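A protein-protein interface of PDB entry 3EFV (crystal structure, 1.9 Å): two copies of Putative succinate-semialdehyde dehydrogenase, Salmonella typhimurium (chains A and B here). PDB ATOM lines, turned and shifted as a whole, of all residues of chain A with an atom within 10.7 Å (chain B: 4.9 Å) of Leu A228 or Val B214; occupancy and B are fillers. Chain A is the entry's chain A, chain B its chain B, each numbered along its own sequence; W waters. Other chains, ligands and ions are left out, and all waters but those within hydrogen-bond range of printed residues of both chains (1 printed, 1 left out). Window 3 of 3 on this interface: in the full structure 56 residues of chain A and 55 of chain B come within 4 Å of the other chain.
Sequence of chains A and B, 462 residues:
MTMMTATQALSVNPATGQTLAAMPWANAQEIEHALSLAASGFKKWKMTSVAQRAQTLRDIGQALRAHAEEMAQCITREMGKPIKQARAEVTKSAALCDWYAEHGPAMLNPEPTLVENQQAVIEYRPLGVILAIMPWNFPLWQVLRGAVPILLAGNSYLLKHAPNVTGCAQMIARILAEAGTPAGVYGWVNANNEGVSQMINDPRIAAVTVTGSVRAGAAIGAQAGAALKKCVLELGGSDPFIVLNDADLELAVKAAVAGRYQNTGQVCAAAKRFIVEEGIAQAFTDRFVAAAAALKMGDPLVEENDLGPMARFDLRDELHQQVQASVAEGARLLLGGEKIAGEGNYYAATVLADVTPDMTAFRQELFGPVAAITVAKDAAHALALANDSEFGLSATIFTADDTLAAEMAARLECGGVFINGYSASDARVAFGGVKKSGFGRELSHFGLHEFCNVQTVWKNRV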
ATOM      1  N   LEU A 127      -5.503 -24.923 -13.197  1.00  0.00           N
ATOM      2  CA  LEU A 127      -5.581 -24.364 -14.549  1.00  0.00           C
ATOM      3  C   LEU A 127      -6.127 -22.940 -14.603  1.00  0.00           C
ATOM      4  O   LEU A 127      -5.595 -22.075 -15.317  1.00  0.00           O
ATOM      5  CB  LEU A 127      -6.469 -25.265 -15.387  1.00  0.00           C
ATOM      6  CG  LEU A 127      -6.358 -25.433 -16.880  1.00  0.00           C
ATOM      7  CD1 LEU A 127      -4.857 -25.539 -17.354  1.00  0.00           C
ATOM      8  CD2 LEU A 127      -7.164 -26.695 -17.289  1.00  0.00           C
ATOM      9  N   VAL A 129     -10.089 -20.601 -14.373  1.00  0.00           N
ATOM     10  CA  VAL A 129     -11.551 -20.604 -14.209  1.00  0.00           C
ATOM     11  C   VAL A 129     -12.126 -21.584 -15.206  1.00  0.00           C
ATOM     12  O   VAL A 129     -11.821 -21.503 -16.401  1.00  0.00           O
ATOM     13  CB  VAL A 129     -12.177 -19.212 -14.448  1.00  0.00           C
ATOM     14  CG1 VAL A 129     -13.697 -19.258 -14.189  1.00  0.00           C
ATOM     15  CG2 VAL A 129     -11.487 -18.156 -13.567  1.00  0.00           C
ATOM     16  N   MET A 199     -18.101 -15.641 -22.948  1.00  0.00           N
ATOM     17  CA  MET A 199     -17.252 -16.186 -21.879  1.00  0.00           C
ATOM     18  C   MET A 199     -16.235 -17.197 -22.402  1.00  0.00           C
ATOM     19  O   MET A 199     -15.062 -17.134 -22.035  1.00  0.00           O
ATOM     20  CB  MET A 199     -18.109 -16.786 -20.754  1.00  0.00           C
ATOM     21  CG  MET A 199     -18.903 -15.715 -20.036  1.00  0.00           C
ATOM     22  SD  MET A 199     -19.815 -16.408 -18.455  1.00  0.00           S
ATOM     23  CE  MET A 199     -21.139 -17.551 -19.334  1.00  0.00           C
ATOM     24  N   ILE A 200     -16.673 -18.104 -23.277  1.00  0.00           N
ATOM     25  CA  ILE A 200     -15.749 -19.092 -23.872  1.00  0.00           C
ATOM     26  C   ILE A 200     -14.576 -18.357 -24.543  1.00  0.00           C
ATOM     27  O   ILE A 200     -13.410 -18.776 -24.453  1.00  0.00           O
ATOM     28  CB  ILE A 200     -16.483 -20.015 -24.880  1.00  0.00           C
ATOM     29  CG1 ILE A 200     -17.515 -20.894 -24.156  1.00  0.00           C
ATOM     30  CG2 ILE A 200     -15.485 -20.918 -25.664  1.00  0.00           C
ATOM     31  CD1 ILE A 200     -18.455 -21.680 -25.151  1.00  0.00           C
ATOM     32  N   ASN A 201     -14.887 -17.236 -25.184  1.00  0.00           N
ATOM     33  CA  ASN A 201     -13.883 -16.455 -25.905  1.00  0.00           C
ATOM     34  C   ASN A 201     -13.094 -15.467 -25.066  1.00  0.00           C
ATOM     35  O   ASN A 201     -12.215 -14.794 -25.581  1.00  0.00           O
ATOM     36  CB  ASN A 201     -14.510 -15.763 -27.115  1.00  0.00           C
ATOM     37  CG  ASN A 201     -14.987 -16.760 -28.150  1.00  0.00           C
ATOM     38  OD1 ASN A 201     -16.163 -16.769 -28.535  1.00  0.00           O
ATOM     39  ND2 ASN A 201     -14.086 -17.628 -28.586  1.00  0.00           N
ATOM     40  N   ASP A 202     -13.363 -15.414 -23.770  1.00  0.00           N
ATOM     41  CA  ASP A 202     -12.645 -14.518 -22.883  1.00  0.00           C
ATOM     42  C   ASP A 202     -11.445 -15.259 -22.284  1.00  0.00           C
ATOM     43  O   ASP A 202     -11.591 -16.397 -21.860  1.00  0.00           O
ATOM     44  CB  ASP A 202     -13.587 -14.046 -21.779  1.00  0.00           C
ATOM     45  CG  ASP A 202     -12.979 -12.966 -20.931  1.00  0.00           C
ATOM     46  OD1 ASP A 202     -12.117 -13.293 -20.092  1.00  0.00           O
ATOM     47  OD2 ASP A 202     -13.381 -11.793 -21.098  1.00  0.00           O
ATOM     48  N   PRO A 203     -10.267 -14.609 -22.238  1.00  0.00           N
ATOM     49  CA  PRO A 203      -9.036 -15.232 -21.726  1.00  0.00           C
ATOM     50  C   PRO A 203      -9.099 -15.693 -20.265  1.00  0.00           C
ATOM     51  O   PRO A 203      -8.335 -16.574 -19.861  1.00  0.00           O
ATOM     52  CB  PRO A 203      -7.972 -14.135 -21.899  1.00  0.00           C
ATOM     53  CG  PRO A 203      -8.689 -12.899 -22.183  1.00  0.00           C
ATOM     54  CD  PRO A 203     -10.041 -13.229 -22.713  1.00  0.00           C
ATOM     55  N   ILE A 205     -11.500 -17.438 -19.005  1.00  0.00           N
ATOM     56  CA  ILE A 205     -11.977 -18.823 -18.988  1.00  0.00           C
ATOM     57  C   ILE A 205     -10.868 -19.747 -19.531  1.00  0.00           C
ATOM     58  O   ILE A 205     -10.427 -19.575 -20.664  1.00  0.00           O
ATOM     59  CB  ILE A 205     -13.313 -19.008 -19.758  1.00  0.00           C
ATOM     60  CG1 ILE A 205     -14.453 -18.230 -19.075  1.00  0.00           C
ATOM     61  CG2 ILE A 205     -13.649 -20.522 -19.903  1.00  0.00           C
ATOM     62  CD1 ILE A 205     -14.640 -18.534 -17.575  1.00  0.00           C
ATOM     63  N   ALA A 206     -10.411 -20.699 -18.704  1.00  0.00           N
ATOM     64  CA  ALA A 206      -9.296 -21.579 -19.088  1.00  0.00           C
ATOM     65  C   ALA A 206      -9.759 -22.823 -19.833  1.00  0.00           C
ATOM     66  O   ALA A 206      -9.075 -23.287 -20.747  1.00  0.00           O
ATOM     67  CB  ALA A 206      -8.497 -21.978 -17.873  1.00  0.00           C
ATOM     68  N   ALA A 207     -10.925 -23.352 -19.442  1.00  0.00           N
ATOM     69  CA  ALA A 207     -11.462 -24.604 -19.999  1.00  0.00           C
ATOM     70  C   ALA A 207     -12.964 -24.659 -19.739  1.00  0.00           C
ATOM     71  O   ALA A 207     -13.509 -23.816 -19.009  1.00  0.00           O
ATOM     72  CB  ALA A 207     -10.780 -25.820 -19.369  1.00  0.00           C
ATOM     73  N   VAL A 208     -13.619 -25.659 -20.327  1.00  0.00           N
ATOM     74  CA  VAL A 208     -15.082 -25.738 -20.314  1.00  0.00           C
ATOM     75  C   VAL A 208     -15.513 -27.157 -20.015  1.00  0.00           C
ATOM     76  O   VAL A 208     -14.896 -28.120 -20.483  1.00  0.00           O
ATOM     77  CB  VAL A 208     -15.666 -25.319 -21.673  1.00  0.00           C
ATOM     78  CG1 VAL A 208     -17.204 -25.344 -21.642  1.00  0.00           C
ATOM     79  CG2 VAL A 208     -15.211 -23.931 -22.045  1.00  0.00           C
ATOM     80  N   ILE A 220     -21.086 -26.155 -28.111  1.00  0.00           N
ATOM     81  CA  ILE A 220     -20.102 -25.618 -27.173  1.00  0.00           C
ATOM     82  C   ILE A 220     -18.695 -26.147 -27.481  1.00  0.00           C
ATOM     83  O   ILE A 220     -17.728 -25.388 -27.441  1.00  0.00           O
ATOM     84  CB  ILE A 220     -20.522 -25.883 -25.719  1.00  0.00           C
ATOM     85  CG1 ILE A 220     -21.805 -25.085 -25.432  1.00  0.00           C
ATOM     86  CG2 ILE A 220     -19.422 -25.453 -24.723  1.00  0.00           C
ATOM     87  CD1 ILE A 220     -22.685 -25.739 -24.422  1.00  0.00           C
ATOM     88  N   GLY A 221     -18.600 -27.441 -27.795  1.00  0.00           N
ATOM     89  CA  GLY A 221     -17.314 -28.068 -28.128  1.00  0.00           C
ATOM     90  C   GLY A 221     -16.646 -27.378 -29.296  1.00  0.00           C
ATOM     91  O   GLY A 221     -15.443 -27.151 -29.273  1.00  0.00           O
ATOM     92  N   ALA A 222     -17.437 -27.030 -30.314  1.00  0.00           N
ATOM     93  CA  ALA A 222     -16.930 -26.269 -31.465  1.00  0.00           C
ATOM     94  C   ALA A 222     -16.307 -24.942 -31.042  1.00  0.00           C
ATOM     95  O   ALA A 222     -15.248 -24.555 -31.552  1.00  0.00           O
ATOM     96  CB  ALA A 222     -18.029 -26.038 -32.491  1.00  0.00           C
ATOM     97  N   GLN A 223     -16.957 -24.245 -30.104  1.00  0.00           N
ATOM     98  CA  GLN A 223     -16.475 -22.942 -29.667  1.00  0.00           C
ATOM     99  C   GLN A 223     -15.232 -23.056 -28.802  1.00  0.00           C
ATOM    100  O   GLN A 223     -14.306 -22.248 -28.931  1.00  0.00           O
ATOM    101  CB  GLN A 223     -17.575 -22.181 -28.910  1.00  0.00           C
ATOM    102  CG  GLN A 223     -18.785 -21.874 -29.787  1.00  0.00           C
ATOM    103  CD  GLN A 223     -19.847 -21.128 -29.024  1.00  0.00           C
ATOM    104  OE1 GLN A 223     -19.715 -19.926 -28.775  1.00  0.00           O
ATOM    105  NE2 GLN A 223     -20.902 -21.833 -28.629  1.00  0.00           N
ATOM    106  N   ALA A 224     -15.226 -24.042 -27.907  1.00  0.00           N
ATOM    107  CA  ALA A 224     -14.070 -24.285 -27.056  1.00  0.00           C
ATOM    108  C   ALA A 224     -12.835 -24.626 -27.911  1.00  0.00           C
ATOM    109  O   ALA A 224     -11.781 -24.046 -27.705  1.00  0.00           O
ATOM    110  CB  ALA A 224     -14.371 -25.396 -26.040  1.00  0.00           C
ATOM    111  N   GLY A 225     -12.989 -25.545 -28.872  1.00  0.00           N
ATOM    112  CA  GLY A 225     -11.898 -25.915 -29.797  1.00  0.00           C
ATOM    113  C   GLY A 225     -11.347 -24.704 -30.539  1.00  0.00           C
ATOM    114  O   GLY A 225     -10.129 -24.501 -30.594  1.00  0.00           O
ATOM    115  N   ALA A 226     -12.250 -23.884 -31.078  1.00  0.00           N
ATOM    116  CA  ALA A 226     -11.867 -22.670 -31.782  1.00  0.00           C
ATOM    117  C   ALA A 226     -11.075 -21.688 -30.901  1.00  0.00           C
ATOM    118  O   ALA A 226     -10.206 -20.965 -31.403  1.00  0.00           O
ATOM    119  CB  ALA A 226     -13.107 -21.990 -32.392  1.00  0.00           C
ATOM    120  N   ALA A 227     -11.343 -21.702 -29.594  1.00  0.00           N
ATOM    121  CA  ALA A 227     -10.665 -20.840 -28.639  1.00  0.00           C
ATOM    122  C   ALA A 227      -9.461 -21.520 -27.999  1.00  0.00           C
ATOM    123  O   ALA A 227      -8.835 -20.941 -27.127  1.00  0.00           O
ATOM    124  CB  ALA A 227     -11.643 -20.396 -27.550  1.00  0.00           C
ATOM    125  N   LEU A 228      -9.157 -22.751 -28.421  1.00  0.00           N
ATOM    126  CA  LEU A 228      -7.999 -23.527 -27.910  1.00  0.00           C
ATOM    127  C   LEU A 228      -8.138 -23.913 -26.437  1.00  0.00           C
ATOM    128  O   LEU A 228      -7.160 -23.988 -25.673  1.00  0.00           O
ATOM    129  CB  LEU A 228      -6.659 -22.831 -28.210  1.00  0.00           C
ATOM    130  CG  LEU A 228      -6.572 -22.461 -29.695  1.00  0.00           C
ATOM    131  CD1 LEU A 228      -5.474 -21.489 -29.934  1.00  0.00           C
ATOM    132  CD2 LEU A 228      -6.456 -23.705 -30.573  1.00  0.00           C
ATOM    133  N   LYS A 229      -9.367 -24.223 -26.065  1.00  0.00           N
ATOM    134  CA  LYS A 229      -9.663 -24.554 -24.695  1.00  0.00           C
ATOM    135  C   LYS A 229     -10.194 -25.950 -24.619  1.00  0.00           C
ATOM    136  O   LYS A 229     -11.040 -26.363 -25.424  1.00  0.00           O
ATOM    137  CB  LYS A 229     -10.646 -23.556 -24.101  1.00  0.00           C
ATOM    138  CG  LYS A 229      -9.956 -22.196 -23.914  1.00  0.00           C
ATOM    139  CD  LYS A 229     -10.906 -21.079 -23.601  1.00  0.00           C
ATOM    140  CE  LYS A 229     -10.183 -19.740 -23.842  1.00  0.00           C
ATOM    141  NZ  LYS A 229     -10.983 -18.642 -23.240  1.00  0.00           N
ATOM    142  N   LYS A 230      -9.655 -26.675 -23.654  1.00  0.00           N
ATOM    143  CA  LYS A 230     -10.014 -28.056 -23.438  1.00  0.00           C
ATOM    144  C   LYS A 230     -11.446 -28.134 -22.922  1.00  0.00           C
ATOM    145  O   LYS A 230     -11.908 -27.227 -22.210  1.00  0.00           O
ATOM    146  CB  LYS A 230      -9.094 -28.608 -22.370  1.00  0.00           C
ATOM    147  CG  LYS A 230      -9.099 -30.079 -22.257  1.00  0.00           C
ATOM    148  CD  LYS A 230      -8.806 -30.411 -20.803  1.00  0.00           C
ATOM    149  CE  LYS A 230      -9.295 -31.797 -20.455  1.00  0.00           C
ATOM    150  NZ  LYS A 230      -8.175 -32.725 -20.174  1.00  0.00           N
ATOM    151  N   CYS A 231     -12.119 -29.225 -23.301  1.00  0.00           N
ATOM    152  CA  CYS A 231     -13.465 -29.577 -22.839  1.00  0.00           C
ATOM    153  C   CYS A 231     -13.517 -30.931 -22.158  1.00  0.00           C
ATOM    154  O   CYS A 231     -12.644 -31.793 -22.362  1.00  0.00           O
ATOM    155  CB  CYS A 231     -14.437 -29.679 -24.014  1.00  0.00           C
ATOM    156  SG  CYS A 231     -14.991 -28.155 -24.691  1.00  0.00           S
ATOM    157  N   PHE A 451      -8.905 -31.087 -15.264  1.00  0.00           N
ATOM    158  CA  PHE A 451      -8.732 -29.635 -15.220  1.00  0.00           C
ATOM    159  C   PHE A 451      -7.506 -29.200 -14.414  1.00  0.00           C
ATOM    160  O   PHE A 451      -7.505 -28.148 -13.750  1.00  0.00           O
ATOM    161  CB  PHE A 451     -10.039 -28.938 -14.783  1.00  0.00           C
ATOM    162  CG  PHE A 451     -11.178 -29.224 -15.719  1.00  0.00           C
ATOM    163  CD1 PHE A 451     -11.226 -28.628 -16.966  1.00  0.00           C
ATOM    164  CD2 PHE A 451     -12.144 -30.146 -15.385  1.00  0.00           C
ATOM    165  CE1 PHE A 451     -12.260 -28.923 -17.861  1.00  0.00           C
ATOM    166  CE2 PHE A 451     -13.185 -30.451 -16.276  1.00  0.00           C
ATOM    167  CZ  PHE A 451     -13.232 -29.835 -17.502  1.00  0.00           C
ATOM    168  N   GLY B 212       1.146 -28.283 -34.491  1.00  0.00           N
ATOM    169  CA  GLY B 212       1.183 -27.267 -35.538  1.00  0.00           C
ATOM    170  C   GLY B 212       0.996 -25.867 -34.992  1.00  0.00           C
ATOM    171  O   GLY B 212       1.209 -25.624 -33.798  1.00  0.00           O
ATOM    172  N   SER B 213       0.595 -24.953 -35.863  1.00  0.00           N
ATOM    173  CA  SER B 213       0.417 -23.560 -35.452  1.00  0.00           C
ATOM    174  C   SER B 213      -0.868 -23.392 -34.655  1.00  0.00           C
ATOM    175  O   SER B 213      -1.777 -24.242 -34.703  1.00  0.00           O
ATOM    176  CB  SER B 213       0.340 -22.660 -36.677  1.00  0.00           C
ATOM    177  OG  SER B 213      -0.823 -22.982 -37.407  1.00  0.00           O
ATOM    178  N   VAL B 214      -0.953 -22.268 -33.951  1.00  0.00           N
ATOM    179  CA  VAL B 214      -2.214 -21.844 -33.313  1.00  0.00           C
ATOM    180  C   VAL B 214      -3.396 -21.839 -34.302  1.00  0.00           C
ATOM    181  O   VAL B 214      -4.467 -22.363 -33.975  1.00  0.00           O
ATOM    182  CB  VAL B 214      -2.042 -20.455 -32.607  1.00  0.00           C
ATOM    183  CG1 VAL B 214      -3.362 -19.940 -32.086  1.00  0.00           C
ATOM    184  CG2 VAL B 214      -1.050 -20.572 -31.462  1.00  0.00           C
ATOM    185  N   ARG B 215      -3.214 -21.271 -35.503  1.00  0.00           N
ATOM    186  CA  ARG B 215      -4.304 -21.209 -36.489  1.00  0.00           C
ATOM    187  C   ARG B 215      -4.803 -22.580 -36.889  1.00  0.00           C
ATOM    188  O   ARG B 215      -5.998 -22.781 -37.007  1.00  0.00           O
ATOM    189  CB  ARG B 215      -3.904 -20.473 -37.777  1.00  0.00           C
ATOM    190  CG  ARG B 215      -3.609 -18.996 -37.629  1.00  0.00           C
ATOM    191  CD  ARG B 215      -3.209 -18.441 -39.017  1.00  0.00           C
ATOM    192  NE  ARG B 215      -4.338 -18.522 -39.949  1.00  0.00           N
ATOM    193  CZ  ARG B 215      -4.248 -18.478 -41.280  1.00  0.00           C
ATOM    194  NH1 ARG B 215      -3.062 -18.376 -41.894  1.00  0.00           N
ATOM    195  NH2 ARG B 215      -5.363 -18.537 -42.005  1.00  0.00           N
ATOM    196  N   ALA B 216      -3.878 -23.510 -37.128  1.00  0.00           N
ATOM    197  CA  ALA B 216      -4.227 -24.877 -37.477  1.00  0.00           C
ATOM    198  C   ALA B 216      -4.993 -25.546 -36.335  1.00  0.00           C
ATOM    199  O   ALA B 216      -6.011 -26.208 -36.564  1.00  0.00           O
ATOM    200  CB  ALA B 216      -2.972 -25.681 -37.803  1.00  0.00           C
ATOM    201  N   GLY B 217      -4.481 -25.396 -35.117  1.00  0.00           N
ATOM    202  CA  GLY B 217      -5.108 -25.967 -33.930  1.00  0.00           C
ATOM    203  C   GLY B 217      -6.541 -25.473 -33.763  1.00  0.00           C
ATOM    204  O   GLY B 217      -7.448 -26.265 -33.464  1.00  0.00           O
ATOM    205  N   ALA B 218      -6.758 -24.174 -33.976  1.00  0.00           N
ATOM    206  CA  ALA B 218      -8.105 -23.611 -33.819  1.00  0.00           C
ATOM    207  C   ALA B 218      -9.029 -24.111 -34.917  1.00  0.00           C
ATOM    208  O   ALA B 218     -10.195 -24.409 -34.654  1.00  0.00           O
ATOM    209  CB  ALA B 218      -8.080 -22.081 -33.789  1.00  0.00           C
ATOM    210  N   LEU B 233      -4.044 -30.912 -28.701  1.00  0.00           N
ATOM    211  CA  LEU B 233      -3.535 -29.837 -29.539  1.00  0.00           C
ATOM    212  C   LEU B 233      -2.203 -29.386 -28.964  1.00  0.00           C
ATOM    213  O   LEU B 233      -2.157 -28.859 -27.842  1.00  0.00           O
ATOM    214  CB  LEU B 233      -4.511 -28.660 -29.570  1.00  0.00           C
ATOM    215  CG  LEU B 233      -5.933 -28.926 -30.071  1.00  0.00           C
ATOM    216  CD1 LEU B 233      -6.727 -27.590 -30.039  1.00  0.00           C
ATOM    217  CD2 LEU B 233      -5.941 -29.544 -31.501  1.00  0.00           C
ATOM    218  N   LEU B 235       0.557 -26.940 -29.780  1.00  0.00           N
ATOM    219  CA  LEU B 235       0.652 -25.829 -30.698  1.00  0.00           C
ATOM    220  C   LEU B 235       1.891 -24.990 -30.389  1.00  0.00           C
ATOM    221  O   LEU B 235       2.827 -25.476 -29.733  1.00  0.00           O
ATOM    222  CB  LEU B 235      -0.663 -25.018 -30.691  1.00  0.00           C
ATOM    223  CG  LEU B 235      -1.943 -25.871 -30.853  1.00  0.00           C
ATOM    224  CD1 LEU B 235      -3.206 -25.003 -30.671  1.00  0.00           C
ATOM    225  CD2 LEU B 235      -1.975 -26.644 -32.201  1.00  0.00           C
ATOM    226  N   GLY B 236       1.939 -23.758 -30.866  1.00  0.00           N
ATOM    227  CA  GLY B 236       3.190 -23.009 -30.731  1.00  0.00           C
ATOM    228  C   GLY B 236       3.562 -22.625 -29.302  1.00  0.00           C
ATOM    229  O   GLY B 236       2.761 -22.779 -28.362  1.00  0.00           O
ATOM    230  N   PHE B 391       0.930 -17.638 -24.942  1.00  0.00           N
ATOM    231  CA  PHE B 391       1.463 -19.007 -25.041  1.00  0.00           C
ATOM    232  C   PHE B 391       1.832 -19.521 -23.662  1.00  0.00           C
ATOM    233  O   PHE B 391       2.015 -18.739 -22.724  1.00  0.00           O
ATOM    234  CB  PHE B 391       2.725 -19.016 -25.929  1.00  0.00           C
ATOM    235  CG  PHE B 391       2.468 -18.546 -27.337  1.00  0.00           C
ATOM    236  CD1 PHE B 391       1.985 -19.436 -28.302  1.00  0.00           C
ATOM    237  CD2 PHE B 391       2.673 -17.208 -27.689  1.00  0.00           C
ATOM    238  CE1 PHE B 391       1.726 -18.998 -29.610  1.00  0.00           C
ATOM    239  CE2 PHE B 391       2.413 -16.762 -28.999  1.00  0.00           C
ATOM    240  CZ  PHE B 391       1.936 -17.656 -29.952  1.00  0.00           C
ATOM    241  N   LYS B 435      -3.012 -22.304 -22.268  1.00  0.00           N
ATOM    242  CA  LYS B 435      -3.341 -21.117 -23.058  1.00  0.00           C
ATOM    243  C   LYS B 435      -3.305 -21.448 -24.556  1.00  0.00           C
ATOM    244  O   LYS B 435      -3.794 -22.522 -24.946  1.00  0.00           O
ATOM    245  CB  LYS B 435      -2.416 -19.943 -22.719  1.00  0.00           C
ATOM    246  CG  LYS B 435      -2.425 -19.521 -21.249  1.00  0.00           C
ATOM    247  CD  LYS B 435      -1.327 -18.481 -21.029  1.00  0.00           C
ATOM    248  CE  LYS B 435      -1.193 -18.085 -19.582  1.00  0.00           C
ATOM    249  NZ  LYS B 435      -0.008 -17.144 -19.406  1.00  0.00           N
ATOM    250  N   LYS B 436      -2.753 -20.567 -25.404  1.00  0.00           N
ATOM    251  CA  LYS B 436      -2.832 -20.826 -26.845  1.00  0.00           C
ATOM    252  C   LYS B 436      -1.839 -21.880 -27.340  1.00  0.00           C
ATOM    253  O   LYS B 436      -1.849 -22.239 -28.522  1.00  0.00           O
ATOM    254  CB  LYS B 436      -2.733 -19.547 -27.681  1.00  0.00           C
ATOM    255  CG  LYS B 436      -3.920 -18.606 -27.453  1.00  0.00           C
ATOM    256  CD  LYS B 436      -3.919 -17.510 -28.505  1.00  0.00           C
ATOM    257  CE  LYS B 436      -5.063 -16.520 -28.295  1.00  0.00           C
ATOM    258  NZ  LYS B 436      -6.385 -17.199 -28.224  1.00  0.00           N
ATOM    259  N   GLY B 438      -2.253 -24.786 -26.461  1.00  0.00           N
ATOM    260  CA  GLY B 438      -3.196 -25.885 -26.712  1.00  0.00           C
ATOM    261  C   GLY B 438      -3.624 -26.566 -25.422  1.00  0.00           C
ATOM    262  O   GLY B 438      -3.837 -25.912 -24.395  1.00  0.00           O
ATOM    263  N   PHE B 439      -3.742 -27.888 -25.470  1.00  0.00           N
ATOM    264  CA  PHE B 439      -4.160 -28.657 -24.314  1.00  0.00           C
ATOM    265  C   PHE B 439      -3.927 -30.136 -24.586  1.00  0.00           C
ATOM    266  O   PHE B 439      -3.749 -30.540 -25.734  1.00  0.00           O
ATOM    267  CB  PHE B 439      -5.644 -28.387 -23.955  1.00  0.00           C
ATOM    268  CG  PHE B 439      -6.606 -28.599 -25.097  1.00  0.00           C
ATOM    269  CD1 PHE B 439      -7.009 -29.890 -25.471  1.00  0.00           C
ATOM    270  CD2 PHE B 439      -7.141 -27.502 -25.775  1.00  0.00           C
ATOM    271  CE1 PHE B 439      -7.908 -30.083 -26.516  1.00  0.00           C
ATOM    272  CE2 PHE B 439      -8.042 -27.679 -26.835  1.00  0.00           C
ATOM    273  CZ  PHE B 439      -8.424 -28.971 -27.210  1.00  0.00           C
HETATM  274  O   HOH W   1      -8.917 -18.158 -27.042  1.00  0.00           O
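NZ of Lys A229 lies within hydrogen-bond range of O of Ile A200, at 2.7 Å. NZ of Lys A229 lies within hydrogen-bond range of O of Asp A202 (2.7 Å). The backbone carbonyl oxygen of Ile A205 lies within hydrogen-bond range of the side-chain amino group of Lys A229, 2.8 Å away. The backbone NH (N) of Val A208 is in hydrogen-bond range of the backbone carbonyl oxygen (O) of Lys A230. The backbone carbonyl oxygen (O) of Ala A224 sits at hydrogen-bond distance from the backbone NH (N) of Lys A229 (2.9 Å). The backbone carbonyl oxygen of Phe B439 lies within hydrogen-bond range of the backbone NH of Leu B233, at 3.0 Å.
O of Gly A225 touches CA of Ala B218 (3.9 Å). O of Ala A226 touches CB of Ala B218, 3.4 Å away. Leu A228 touches Val B214. C of Gly B217 touches CD2 of Leu A228 (3.6 Å). Leu A228 touches Ala B218. Leu A228 touches Leu B233. Leu A228 touches Lys B435 (O to O, 3.7 Å). CD2 of Phe B439 touches O of Leu A228, 3.5 Å away. Phe B439 touches Lys A229 (CE2 to C, 3.5 Å). Phe B439 touches Lys A230 (CD2 to N, 3.4 Å).
Of chain A, only Leu A228 comes within 4 Å of Val B214. No residue of chain A comes within 4 Å of Ser B213. No residue of chain A comes within 4 Å of Ala B216. Gly B217 touches one residue of chain A. Ala B218 touches three residues of chain A. Leu B235 touches just one residue of chain A: Leu A228. No residue of chain A comes within 4 Å of Gly B236. Lys B436 touches just one residue of chain A: Leu A228 (3.96 Å). Of the printed residues of chain A, Lys B435 touches Leu A228. Printed residues of chain B within 4 Å of Lys A229: Phe B439. Ile A205 touches none of the printed residues of chain B. The nearest printed residue of chain B that does not touch Lys A230 is Gly B438 (5.9 Å).
Of the 24 printed residues of chain A, 5 touch a printed residue of chain B. Hydrophobic or aromatic side chains of chain A that line the printed part of chain B: Leu A228. Of the 15 printed residues of chain B, 8 touch a printed residue of chain A. Hydrophobic or aromatic side chains of chain B that line the printed part of chain A: Val B214, Ala B218, Leu B233, Leu B235 and Phe B439. Among the printed residues, no Asp or Glu carboxylate lies within 4 Å of a Lys or Arg side-chain nitrogen of the other chain.
No position is printed for both chains. Of the 12 pairs that touch across the chains among the printed residues, none has its exchanged pair printed and touching as well.
Water W1 bridges O of Ala A227 (2.8 Å) and NZ of Lys B436 (3.0 Å).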
